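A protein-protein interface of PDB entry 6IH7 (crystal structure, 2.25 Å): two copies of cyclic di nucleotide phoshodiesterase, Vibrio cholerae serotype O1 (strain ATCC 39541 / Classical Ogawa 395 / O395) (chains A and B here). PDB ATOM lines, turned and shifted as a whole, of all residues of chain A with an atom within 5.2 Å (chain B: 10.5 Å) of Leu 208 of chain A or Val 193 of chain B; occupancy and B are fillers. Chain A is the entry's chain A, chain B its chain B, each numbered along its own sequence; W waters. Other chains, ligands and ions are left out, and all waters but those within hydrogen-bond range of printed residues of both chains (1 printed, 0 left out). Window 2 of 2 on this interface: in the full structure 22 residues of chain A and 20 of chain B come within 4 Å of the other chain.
The backbone carbonyl oxygen of Ala 171 of chain A sits at hydrogen-bond distance from the guanidinium group of Arg 194 of chain B, at 3.2 Å. The side-chain carboxylate (OD2) of Asp 207 of chain A lies within hydrogen-bond range of the side-chain hydroxyl (OG) of Ser 196 of chain B, 2.9 Å away. The side-chain carboxylate (OD2) of Asp 207 of chain A is in hydrogen-bond range of the side-chain amide nitrogen (ND2) of Asn 200 of chain B (2.9 Å).
The backbone carbonyl oxygen (O) of Gly 183 of chain B lies within hydrogen-bond range of the guanidinium group (NE) of Arg 194 of chain B (2.8 Å). OD1 of Asp 191 of chain B is in hydrogen-bond range of N of Val 193 of chain B. The side-chain carboxylate (OD2) of Asp 191 of chain B is in salt-bridge range of the guanidinium group (NH1) of Arg 194 of chain B. The backbone carbonyl oxygen of Ile 197 of chain B sits at hydrogen-bond distance from the side-chain sulfur of Cys 201 of chain B, at 3.3 Å. O of Leu 170 of chain A is in hydrogen-bond range of NE2 of Gln 174 of chain A (2.7 Å). The side-chain carboxylate (OD1) of Asp 207 of chain A lies within salt-bridge range of the side-chain amino group (NZ) of Lys 203 of chain A, 2.8 Å away.
Leu 170 of chain A touches Val 193 of chain B (O to CG1, 3.4 Å). CD2 of Leu 184 of chain B touches CB of Ala 171 of chain A (3.7 Å). O of Ala 171 of chain A touches CG1 of Val 193 of chain B, 3.7 Å away. Ala 171 of chain A touches Ile 197 of chain B. Val 193 of chain B touches Gln 174 of chain A (CG1 to NE2, 3.6 Å). Asn 200 of chain B touches Lys 203 of chain A (OD1 to CD, 3.6 Å). CD1 of Leu 204 of chain A touches OG of Ser 196 of chain B (3.6 Å). Ile 197 of chain B touches Leu 204 of chain A (N to CD1, 3.6 Å). Asn 200 of chain B touches Leu 204 of chain A. Leu 208 of chain A touches Val 193 of chain B.
No position is printed for both chains.
Of the 11 printed residues of chain A, 7 touch a printed residue of chain B. Printed residues of chain A that touch a printed residue of chain B: Leu 170, Ala 171, Gln 174, Lys 203, Leu 204, Asp 207 and Leu 208. Hydrophobic or aromatic side chains of chain A within 4 Å of the printed part of chain B: Ala 171, Leu 204 and Leu 208. Among the printed residues, no Asp or Glu carboxylate lies within 4 Å of a Lys or Arg side-chain nitrogen of the other chain.
Leu 208 of chain A touches just one residue of chain B: Val 193 (3.9 Å). Asp 207 of chain A touches two residues of chain B. No residue of chain B comes within 4 Å of Asn 209 of chain A. No residue of chain B comes within 4 Å of Ile 210 of chain A. Of the printed residues of chain A, Ile 197 of chain B touches Ala 171 and Leu 204. Of the printed residues of chain A, Ser 196 of chain B touches Leu 204 and Asp 207. Printed residues of chain A within 4 Å of Leu 184 of chain B: Ala 171. Printed residues of chain B within 4 Å of Gln 174 of chain A: Val 193. Printed residues of chain A within 4 Å of Asn 200 of chain B: Lys 203, Leu 204 and Asp 207. Arg 186 of chain B touches none of the printed residues of chain A. The nearest residue of chain A that does not touch Val 193 of chain B is Leu 204 of chain A (5.1 Å). The nearest printed residue of chain A that does not touch Ile 197 of chain B is Leu 170 of chain A (4.2 Å).
Water W1 lies within hydrogen-bond range of OD1 of Asp 191 of chain B and O of Ala 171 of chain A.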
ATOM      1  N   LEU A 170      12.427 -16.491  13.467  1.00  0.00           N
ATOM      2  CA  LEU A 170      11.059 -15.994  13.339  1.00  0.00           C
ATOM      3  C   LEU A 170      10.022 -17.009  13.811  1.00  0.00           C
ATOM      4  O   LEU A 170       8.912 -16.623  14.197  1.00  0.00           O
ATOM      5  CB  LEU A 170      10.765 -15.631  11.890  1.00  0.00           C
ATOM      6  CG  LEU A 170      11.247 -14.289  11.395  1.00  0.00           C
ATOM      7  CD1 LEU A 170      10.700 -14.066   9.994  1.00  0.00           C
ATOM      8  CD2 LEU A 170      10.771 -13.214  12.373  1.00  0.00           C
ATOM      9  N   ALA A 171      10.349 -18.307  13.742  1.00  0.00           N
ATOM     10  CA  ALA A 171       9.366 -19.340  14.035  1.00  0.00           C
ATOM     11  C   ALA A 171       9.001 -19.363  15.515  1.00  0.00           C
ATOM     12  O   ALA A 171       7.852 -19.654  15.861  1.00  0.00           O
ATOM     13  CB  ALA A 171       9.891 -20.715  13.581  1.00  0.00           C
ATOM     14  N   GLN A 174       8.937 -13.187  17.635  1.00  0.00           N
ATOM     15  CA  GLN A 174       8.761 -12.126  16.653  1.00  0.00           C
ATOM     16  C   GLN A 174       9.153 -10.791  17.269  1.00  0.00           C
ATOM     17  O   GLN A 174       8.711 -10.443  18.366  1.00  0.00           O
ATOM     18  CB  GLN A 174       7.317 -12.076  16.125  1.00  0.00           C
ATOM     19  CG  GLN A 174       6.913 -13.300  15.286  1.00  0.00           C
ATOM     20  CD  GLN A 174       6.491 -14.456  16.156  1.00  0.00           C
ATOM     21  OE1 GLN A 174       5.625 -14.299  17.014  1.00  0.00           O
ATOM     22  NE2 GLN A 174       7.128 -15.608  15.983  1.00  0.00           N
ATOM     23  N   LYS A 203       5.872 -10.549   2.317  1.00  0.00           N
ATOM     24  CA  LYS A 203       4.516 -10.979   2.636  1.00  0.00           C
ATOM     25  C   LYS A 203       4.490 -11.785   3.938  1.00  0.00           C
ATOM     26  O   LYS A 203       3.552 -11.662   4.733  1.00  0.00           O
ATOM     27  CB  LYS A 203       3.943 -11.793   1.466  1.00  0.00           C
ATOM     28  CG  LYS A 203       2.458 -11.571   1.215  1.00  0.00           C
ATOM     29  CD  LYS A 203       1.648 -12.486   2.105  1.00  0.00           C
ATOM     30  CE  LYS A 203       0.159 -12.104   2.124  1.00  0.00           C
ATOM     31  NZ  LYS A 203      -0.648 -13.099   2.937  1.00  0.00           N
ATOM     32  N   LEU A 204       5.508 -12.616   4.172  1.00  0.00           N
ATOM     33  CA  LEU A 204       5.628 -13.276   5.467  1.00  0.00           C
ATOM     34  C   LEU A 204       5.737 -12.256   6.611  1.00  0.00           C
ATOM     35  O   LEU A 204       5.080 -12.412   7.651  1.00  0.00           O
ATOM     36  CB  LEU A 204       6.838 -14.200   5.457  1.00  0.00           C
ATOM     37  CG  LEU A 204       7.298 -14.675   6.832  1.00  0.00           C
ATOM     38  CD1 LEU A 204       6.317 -15.645   7.436  1.00  0.00           C
ATOM     39  CD2 LEU A 204       8.684 -15.279   6.727  1.00  0.00           C
ATOM     40  N   PHE A 205       6.592 -11.233   6.456  1.00  0.00           N
ATOM     41  CA  PHE A 205       6.727 -10.203   7.497  1.00  0.00           C
ATOM     42  C   PHE A 205       5.412  -9.484   7.719  1.00  0.00           C
ATOM     43  O   PHE A 205       5.033  -9.194   8.863  1.00  0.00           O
ATOM     44  CB  PHE A 205       7.800  -9.168   7.138  1.00  0.00           C
ATOM     45  CG  PHE A 205       9.170  -9.734   7.007  1.00  0.00           C
ATOM     46  CD1 PHE A 205       9.547 -10.852   7.734  1.00  0.00           C
ATOM     47  CD2 PHE A 205      10.091  -9.162   6.128  1.00  0.00           C
ATOM     48  CE1 PHE A 205      10.825 -11.388   7.587  1.00  0.00           C
ATOM     49  CE2 PHE A 205      11.350  -9.697   5.992  1.00  0.00           C
ATOM     50  CZ  PHE A 205      11.721 -10.813   6.717  1.00  0.00           C
ATOM     51  N   SER A 206       4.703  -9.184   6.632  1.00  0.00           N
ATOM     52  CA  SER A 206       3.357  -8.633   6.747  1.00  0.00           C
ATOM     53  C   SER A 206       2.432  -9.540   7.562  1.00  0.00           C
ATOM     54  O   SER A 206       1.683  -9.057   8.421  1.00  0.00           O
ATOM     55  CB  SER A 206       2.784  -8.408   5.360  1.00  0.00           C
ATOM     56  OG  SER A 206       1.605  -7.655   5.470  1.00  0.00           O
ATOM     57  N   ASP A 207       2.437 -10.858   7.285  1.00  0.00           N
ATOM     58  CA  ASP A 207       1.504 -11.760   7.970  1.00  0.00           C
ATOM     59  C   ASP A 207       1.765 -11.782   9.470  1.00  0.00           C
ATOM     60  O   ASP A 207       0.831 -11.814  10.277  1.00  0.00           O
ATOM     61  CB  ASP A 207       1.616 -13.194   7.433  1.00  0.00           C
ATOM     62  CG  ASP A 207       1.175 -13.336   5.989  1.00  0.00           C
ATOM     63  OD1 ASP A 207       0.418 -12.480   5.480  1.00  0.00           O
ATOM     64  OD2 ASP A 207       1.596 -14.327   5.362  1.00  0.00           O
ATOM     65  N   LEU A 208       3.035 -11.774   9.850  1.00  0.00           N
ATOM     66  CA  LEU A 208       3.480 -11.749  11.229  1.00  0.00           C
ATOM     67  C   LEU A 208       3.460 -10.346  11.826  1.00  0.00           C
ATOM     68  O   LEU A 208       3.814 -10.185  12.996  1.00  0.00           O
ATOM     69  CB  LEU A 208       4.893 -12.338  11.307  1.00  0.00           C
ATOM     70  CG  LEU A 208       5.050 -13.764  10.740  1.00  0.00           C
ATOM     71  CD1 LEU A 208       6.456 -14.329  10.965  1.00  0.00           C
ATOM     72  CD2 LEU A 208       3.986 -14.676  11.346  1.00  0.00           C
ATOM     73  N   ASN A 209       3.084  -9.336  11.043  1.00  0.00           N
ATOM     74  CA  ASN A 209       2.990  -7.958  11.518  1.00  0.00           C
ATOM     75  C   ASN A 209       4.341  -7.459  12.008  1.00  0.00           C
ATOM     76  O   ASN A 209       4.453  -6.866  13.078  1.00  0.00           O
ATOM     77  CB  ASN A 209       1.927  -7.820  12.608  1.00  0.00           C
ATOM     78  CG  ASN A 209       0.808  -6.888  12.201  1.00  0.00           C
ATOM     79  OD1 ASN A 209       0.957  -5.657  12.244  1.00  0.00           O
ATOM     80  ND2 ASN A 209      -0.324  -7.467  11.792  1.00  0.00           N
ATOM     81  N   ILE A 210       5.378  -7.758  11.236  1.00  0.00           N
ATOM     82  CA  ILE A 210       6.737  -7.321  11.493  1.00  0.00           C
ATOM     83  C   ILE A 210       7.079  -6.301  10.429  1.00  0.00           C
ATOM     84  O   ILE A 210       6.782  -6.504   9.239  1.00  0.00           O
ATOM     85  CB  ILE A 210       7.759  -8.469  11.441  1.00  0.00           C
ATOM     86  CG1 ILE A 210       7.452  -9.514  12.495  1.00  0.00           C
ATOM     87  CG2 ILE A 210       9.177  -7.913  11.609  1.00  0.00           C
ATOM     88  CD1 ILE A 210       8.200 -10.770  12.273  1.00  0.00           C
ATOM     89  N   GLY B 183      12.230 -28.533  12.617  1.00  0.00           N
ATOM     90  CA  GLY B 183      11.836 -27.506  13.569  1.00  0.00           C
ATOM     91  C   GLY B 183      10.666 -26.686  13.059  1.00  0.00           C
ATOM     92  O   GLY B 183       9.756 -26.341  13.822  1.00  0.00           O
ATOM     93  N   LEU B 184      10.665 -26.382  11.755  1.00  0.00           N
ATOM     94  CA  LEU B 184       9.601 -25.616  11.112  1.00  0.00           C
ATOM     95  C   LEU B 184       8.342 -26.437  10.870  1.00  0.00           C
ATOM     96  O   LEU B 184       7.272 -25.862  10.633  1.00  0.00           O
ATOM     97  CB  LEU B 184      10.082 -25.051   9.771  1.00  0.00           C
ATOM     98  CG  LEU B 184      11.212 -24.014   9.744  1.00  0.00           C
ATOM     99  CD1 LEU B 184      11.409 -23.403   8.383  1.00  0.00           C
ATOM    100  CD2 LEU B 184      10.902 -22.917  10.775  1.00  0.00           C
ATOM    101  N   ILE B 185       8.444 -27.762  10.898  1.00  0.00           N
ATOM    102  CA  ILE B 185       7.297 -28.598  10.586  1.00  0.00           C
ATOM    103  C   ILE B 185       6.548 -28.970  11.859  1.00  0.00           C
ATOM    104  O   ILE B 185       5.323 -29.130  11.834  1.00  0.00           O
ATOM    105  CB  ILE B 185       7.760 -29.846   9.787  1.00  0.00           C
ATOM    106  CG1 ILE B 185       7.522 -29.606   8.317  1.00  0.00           C
ATOM    107  CG2 ILE B 185       7.114 -31.188  10.300  1.00  0.00           C
ATOM    108  CD1 ILE B 185       7.907 -28.204   7.866  1.00  0.00           C
ATOM    109  N   ARG B 186       7.251 -29.082  12.967  1.00  0.00           N
ATOM    110  CA  ARG B 186       6.644 -29.597  14.188  1.00  0.00           C
ATOM    111  C   ARG B 186       5.410 -28.780  14.574  1.00  0.00           C
ATOM    112  O   ARG B 186       5.467 -27.547  14.707  1.00  0.00           O
ATOM    113  CB  ARG B 186       7.671 -29.607  15.314  1.00  0.00           C
ATOM    114  CG  ARG B 186       7.145 -30.180  16.617  1.00  0.00           C
ATOM    115  CD  ARG B 186       7.030 -31.697  16.540  1.00  0.00           C
ATOM    116  NE  ARG B 186       8.245 -32.309  16.003  1.00  0.00           N
ATOM    117  CZ  ARG B 186       8.333 -32.887  14.797  1.00  0.00           C
ATOM    118  NH1 ARG B 186       7.281 -32.947  13.997  1.00  0.00           N
ATOM    119  NH2 ARG B 186       9.476 -33.399  14.390  1.00  0.00           N
ATOM    120  N   ASN B 187       4.290 -29.483  14.701  1.00  0.00           N
ATOM    121  CA  ASN B 187       3.025 -28.974  15.207  1.00  0.00           C
ATOM    122  C   ASN B 187       2.417 -27.916  14.305  1.00  0.00           C
ATOM    123  O   ASN B 187       1.537 -27.164  14.740  1.00  0.00           O
ATOM    124  CB  ASN B 187       3.192 -28.479  16.650  1.00  0.00           C
ATOM    125  CG  ASN B 187       3.164 -29.635  17.625  1.00  0.00           C
ATOM    126  OD1 ASN B 187       2.516 -30.633  17.338  1.00  0.00           O
ATOM    127  ND2 ASN B 187       3.875 -29.541  18.737  1.00  0.00           N
ATOM    128  N   ILE B 188       2.826 -27.901  13.029  1.00  0.00           N
ATOM    129  CA  ILE B 188       2.456 -26.830  12.114  1.00  0.00           C
ATOM    130  C   ILE B 188       0.952 -26.720  11.895  1.00  0.00           C
ATOM    131  O   ILE B 188       0.469 -25.642  11.543  1.00  0.00           O
ATOM    132  CB  ILE B 188       3.188 -27.013  10.771  1.00  0.00           C
ATOM    133  CG1 ILE B 188       3.113 -25.734   9.941  1.00  0.00           C
ATOM    134  CG2 ILE B 188       2.569 -28.162   9.981  1.00  0.00           C
ATOM    135  CD1 ILE B 188       4.135 -25.674   8.863  1.00  0.00           C
ATOM    136  N   HIS B 189       0.188 -27.806  12.107  1.00  0.00           N
ATOM    137  CA  HIS B 189      -1.261 -27.758  11.926  1.00  0.00           C
ATOM    138  C   HIS B 189      -1.945 -26.785  12.886  1.00  0.00           C
ATOM    139  O   HIS B 189      -3.128 -26.453  12.693  1.00  0.00           O
ATOM    140  CB  HIS B 189      -1.868 -29.155  12.120  1.00  0.00           C
ATOM    141  CG  HIS B 189      -1.540 -29.787  13.438  1.00  0.00           C
ATOM    142  ND1 HIS B 189      -0.288 -30.285  13.733  1.00  0.00           N
ATOM    143  CD2 HIS B 189      -2.315 -30.050  14.521  1.00  0.00           C
ATOM    144  CE1 HIS B 189      -0.299 -30.803  14.950  1.00  0.00           C
ATOM    145  NE2 HIS B 189      -1.521 -30.688  15.443  1.00  0.00           N
ATOM    146  N   ALA B 190      -1.261 -26.365  13.947  1.00  0.00           N
ATOM    147  CA  ALA B 190      -1.883 -25.425  14.872  1.00  0.00           C
ATOM    148  C   ALA B 190      -0.911 -24.354  15.374  1.00  0.00           C
ATOM    149  O   ALA B 190      -1.150 -23.756  16.425  1.00  0.00           O
ATOM    150  CB  ALA B 190      -2.500 -26.183  16.043  1.00  0.00           C
ATOM    151  N   ASP B 191       0.170 -24.097  14.646  1.00  0.00           N
ATOM    152  CA  ASP B 191       1.120 -23.035  14.962  1.00  0.00           C
ATOM    153  C   ASP B 191       0.973 -22.029  13.833  1.00  0.00           C
ATOM    154  O   ASP B 191       1.419 -22.282  12.714  1.00  0.00           O
ATOM    155  CB  ASP B 191       2.542 -23.583  15.072  1.00  0.00           C
ATOM    156  CG  ASP B 191       3.550 -22.526  15.393  1.00  0.00           C
ATOM    157  OD1 ASP B 191       3.323 -21.357  15.050  1.00  0.00           O
ATOM    158  OD2 ASP B 191       4.590 -22.870  15.986  1.00  0.00           O
ATOM    159  N   GLN B 192       0.322 -20.903  14.122  1.00  0.00           N
ATOM    160  CA  GLN B 192       0.009 -19.934  13.078  1.00  0.00           C
ATOM    161  C   GLN B 192       1.269 -19.353  12.451  1.00  0.00           C
ATOM    162  O   GLN B 192       1.296 -19.083  11.245  1.00  0.00           O
ATOM    163  CB  GLN B 192      -0.866 -18.822  13.651  1.00  0.00           C
ATOM    164  CG  GLN B 192      -2.217 -19.298  14.165  1.00  0.00           C
ATOM    165  CD  GLN B 192      -3.211 -19.585  13.044  1.00  0.00           C
ATOM    166  OE1 GLN B 192      -3.480 -20.746  12.710  1.00  0.00           O
ATOM    167  NE2 GLN B 192      -3.776 -18.519  12.469  1.00  0.00           N
ATOM    168  N   VAL B 193       2.322 -19.150  13.248  1.00  0.00           N
ATOM    169  CA  VAL B 193       3.552 -18.569  12.710  1.00  0.00           C
ATOM    170  C   VAL B 193       4.222 -19.546  11.737  1.00  0.00           C
ATOM    171  O   VAL B 193       4.573 -19.186  10.604  1.00  0.00           O
ATOM    172  CB  VAL B 193       4.484 -18.137  13.862  1.00  0.00           C
ATOM    173  CG1 VAL B 193       5.864 -17.781  13.345  1.00  0.00           C
ATOM    174  CG2 VAL B 193       3.907 -16.870  14.610  1.00  0.00           C
ATOM    175  N   ARG B 194       4.361 -20.815  12.138  1.00  0.00           N
ATOM    176  CA  ARG B 194       4.976 -21.783  11.234  1.00  0.00           C
ATOM    177  C   ARG B 194       4.135 -21.965   9.979  1.00  0.00           C
ATOM    178  O   ARG B 194       4.677 -22.204   8.893  1.00  0.00           O
ATOM    179  CB  ARG B 194       5.200 -23.106  11.957  1.00  0.00           C
ATOM    180  CG  ARG B 194       6.481 -23.122  12.788  1.00  0.00           C
ATOM    181  CD  ARG B 194       6.523 -24.264  13.815  1.00  0.00           C
ATOM    182  NE  ARG B 194       7.862 -24.423  14.381  1.00  0.00           N
ATOM    183  CZ  ARG B 194       8.348 -23.731  15.419  1.00  0.00           C
ATOM    184  NH1 ARG B 194       7.609 -22.819  16.076  1.00  0.00           N
ATOM    185  NH2 ARG B 194       9.595 -23.960  15.812  1.00  0.00           N
ATOM    186  N   GLN B 195       2.819 -21.823  10.106  1.00  0.00           N
ATOM    187  CA  GLN B 195       1.938 -21.898   8.952  1.00  0.00           C
ATOM    188  C   GLN B 195       2.266 -20.817   7.941  1.00  0.00           C
ATOM    189  O   GLN B 195       2.409 -21.090   6.734  1.00  0.00           O
ATOM    190  CB  GLN B 195       0.487 -21.801   9.416  1.00  0.00           C
ATOM    191  CG  GLN B 195      -0.021 -23.094   9.993  1.00  0.00           C
ATOM    192  CD  GLN B 195      -1.359 -22.950  10.699  1.00  0.00           C
ATOM    193  OE1 GLN B 195      -2.097 -21.972  10.501  1.00  0.00           O
ATOM    194  NE2 GLN B 195      -1.666 -23.913  11.557  1.00  0.00           N
ATOM    195  N   SER B 196       2.407 -19.577   8.420  1.00  0.00           N
ATOM    196  CA  SER B 196       2.767 -18.473   7.543  1.00  0.00           C
ATOM    197  C   SER B 196       4.167 -18.648   6.974  1.00  0.00           C
ATOM    198  O   SER B 196       4.396 -18.373   5.785  1.00  0.00           O
ATOM    199  CB  SER B 196       2.635 -17.141   8.310  1.00  0.00           C
ATOM    200  OG  SER B 196       2.789 -16.060   7.424  1.00  0.00           O
ATOM    201  N   ILE B 197       5.132 -19.059   7.805  1.00  0.00           N
ATOM    202  CA  ILE B 197       6.480 -19.319   7.293  1.00  0.00           C
ATOM    203  C   ILE B 197       6.422 -20.323   6.146  1.00  0.00           C
ATOM    204  O   ILE B 197       6.974 -20.102   5.057  1.00  0.00           O
ATOM    205  CB  ILE B 197       7.401 -19.822   8.418  1.00  0.00           C
ATOM    206  CG1 ILE B 197       7.673 -18.719   9.440  1.00  0.00           C
ATOM    207  CG2 ILE B 197       8.701 -20.381   7.849  1.00  0.00           C
ATOM    208  CD1 ILE B 197       8.741 -19.092  10.457  1.00  0.00           C
ATOM    209  N   MET B 198       5.708 -21.431   6.362  1.00  0.00           N
ATOM    210  CA  MET B 198       5.658 -22.457   5.338  1.00  0.00           C
ATOM    211  C   MET B 198       4.878 -21.989   4.117  1.00  0.00           C
ATOM    212  O   MET B 198       5.325 -22.189   2.989  1.00  0.00           O
ATOM    213  CB  MET B 198       5.077 -23.742   5.923  1.00  0.00           C
ATOM    214  CG  MET B 198       4.933 -24.884   4.911  1.00  0.00           C
ATOM    215  SD  MET B 198       6.471 -25.684   4.389  1.00  0.00           S
ATOM    216  CE  MET B 198       7.513 -25.440   5.808  1.00  0.00           C
ATOM    217  N   LYS B 199       3.735 -21.325   4.314  1.00  0.00           N
ATOM    218  CA  LYS B 199       2.967 -20.843   3.170  1.00  0.00           C
ATOM    219  C   LYS B 199       3.813 -19.941   2.279  1.00  0.00           C
ATOM    220  O   LYS B 199       3.809 -20.077   1.047  1.00  0.00           O
ATOM    221  CB  LYS B 199       1.723 -20.092   3.647  1.00  0.00           C
ATOM    222  CG  LYS B 199       0.638 -19.944   2.583  1.00  0.00           C
ATOM    223  CD  LYS B 199       0.737 -18.672   1.779  1.00  0.00           C
ATOM    224  CE  LYS B 199      -0.252 -17.628   2.283  1.00  0.00           C
ATOM    225  NZ  LYS B 199      -1.664 -18.026   2.043  1.00  0.00           N
ATOM    226  N   ASN B 200       4.555 -19.007   2.884  1.00  0.00           N
ATOM    227  CA  ASN B 200       5.318 -18.076   2.064  1.00  0.00           C
ATOM    228  C   ASN B 200       6.594 -18.723   1.507  1.00  0.00           C
ATOM    229  O   ASN B 200       7.034 -18.372   0.407  1.00  0.00           O
ATOM    230  CB  ASN B 200       5.562 -16.788   2.870  1.00  0.00           C
ATOM    231  CG  ASN B 200       4.245 -16.009   3.110  1.00  0.00           C
ATOM    232  OD1 ASN B 200       3.665 -15.476   2.182  1.00  0.00           O
ATOM    233  ND2 ASN B 200       3.743 -16.034   4.332  1.00  0.00           N
ATOM    234  N   CYS B 201       7.169 -19.709   2.205  1.00  0.00           N
ATOM    235  CA  CYS B 201       8.321 -20.422   1.646  1.00  0.00           C
ATOM    236  C   CYS B 201       7.936 -21.300   0.447  1.00  0.00           C
ATOM    237  O   CYS B 201       8.656 -21.335  -0.562  1.00  0.00           O
ATOM    238  CB  CYS B 201       9.006 -21.254   2.727  1.00  0.00           C
ATOM    239  SG  CYS B 201      10.031 -20.218   3.828  1.00  0.00           S
ATOM    240  N   TRP B 225      -1.855 -31.336   7.215  1.00  0.00           N
ATOM    241  CA  TRP B 225      -1.677 -29.925   6.899  1.00  0.00           C
ATOM    242  C   TRP B 225      -0.668 -29.740   5.776  1.00  0.00           C
ATOM    243  O   TRP B 225      -0.900 -28.966   4.843  1.00  0.00           O
ATOM    244  CB  TRP B 225      -1.222 -29.145   8.136  1.00  0.00           C
ATOM    245  CG  TRP B 225      -1.324 -27.679   7.933  1.00  0.00           C
ATOM    246  CD1 TRP B 225      -2.378 -26.885   8.287  1.00  0.00           C
ATOM    247  CD2 TRP B 225      -0.357 -26.805   7.306  1.00  0.00           C
ATOM    248  NE1 TRP B 225      -2.132 -25.593   7.934  1.00  0.00           N
ATOM    249  CE2 TRP B 225      -0.904 -25.504   7.330  1.00  0.00           C
ATOM    250  CE3 TRP B 225       0.907 -26.998   6.730  1.00  0.00           C
ATOM    251  CZ2 TRP B 225      -0.233 -24.389   6.799  1.00  0.00           C
ATOM    252  CZ3 TRP B 225       1.581 -25.879   6.205  1.00  0.00           C
ATOM    253  CH2 TRP B 225       1.006 -24.590   6.258  1.00  0.00           C
HETATM  254  O   HOH W   1       5.027 -20.011  17.155  1.00  0.00           O
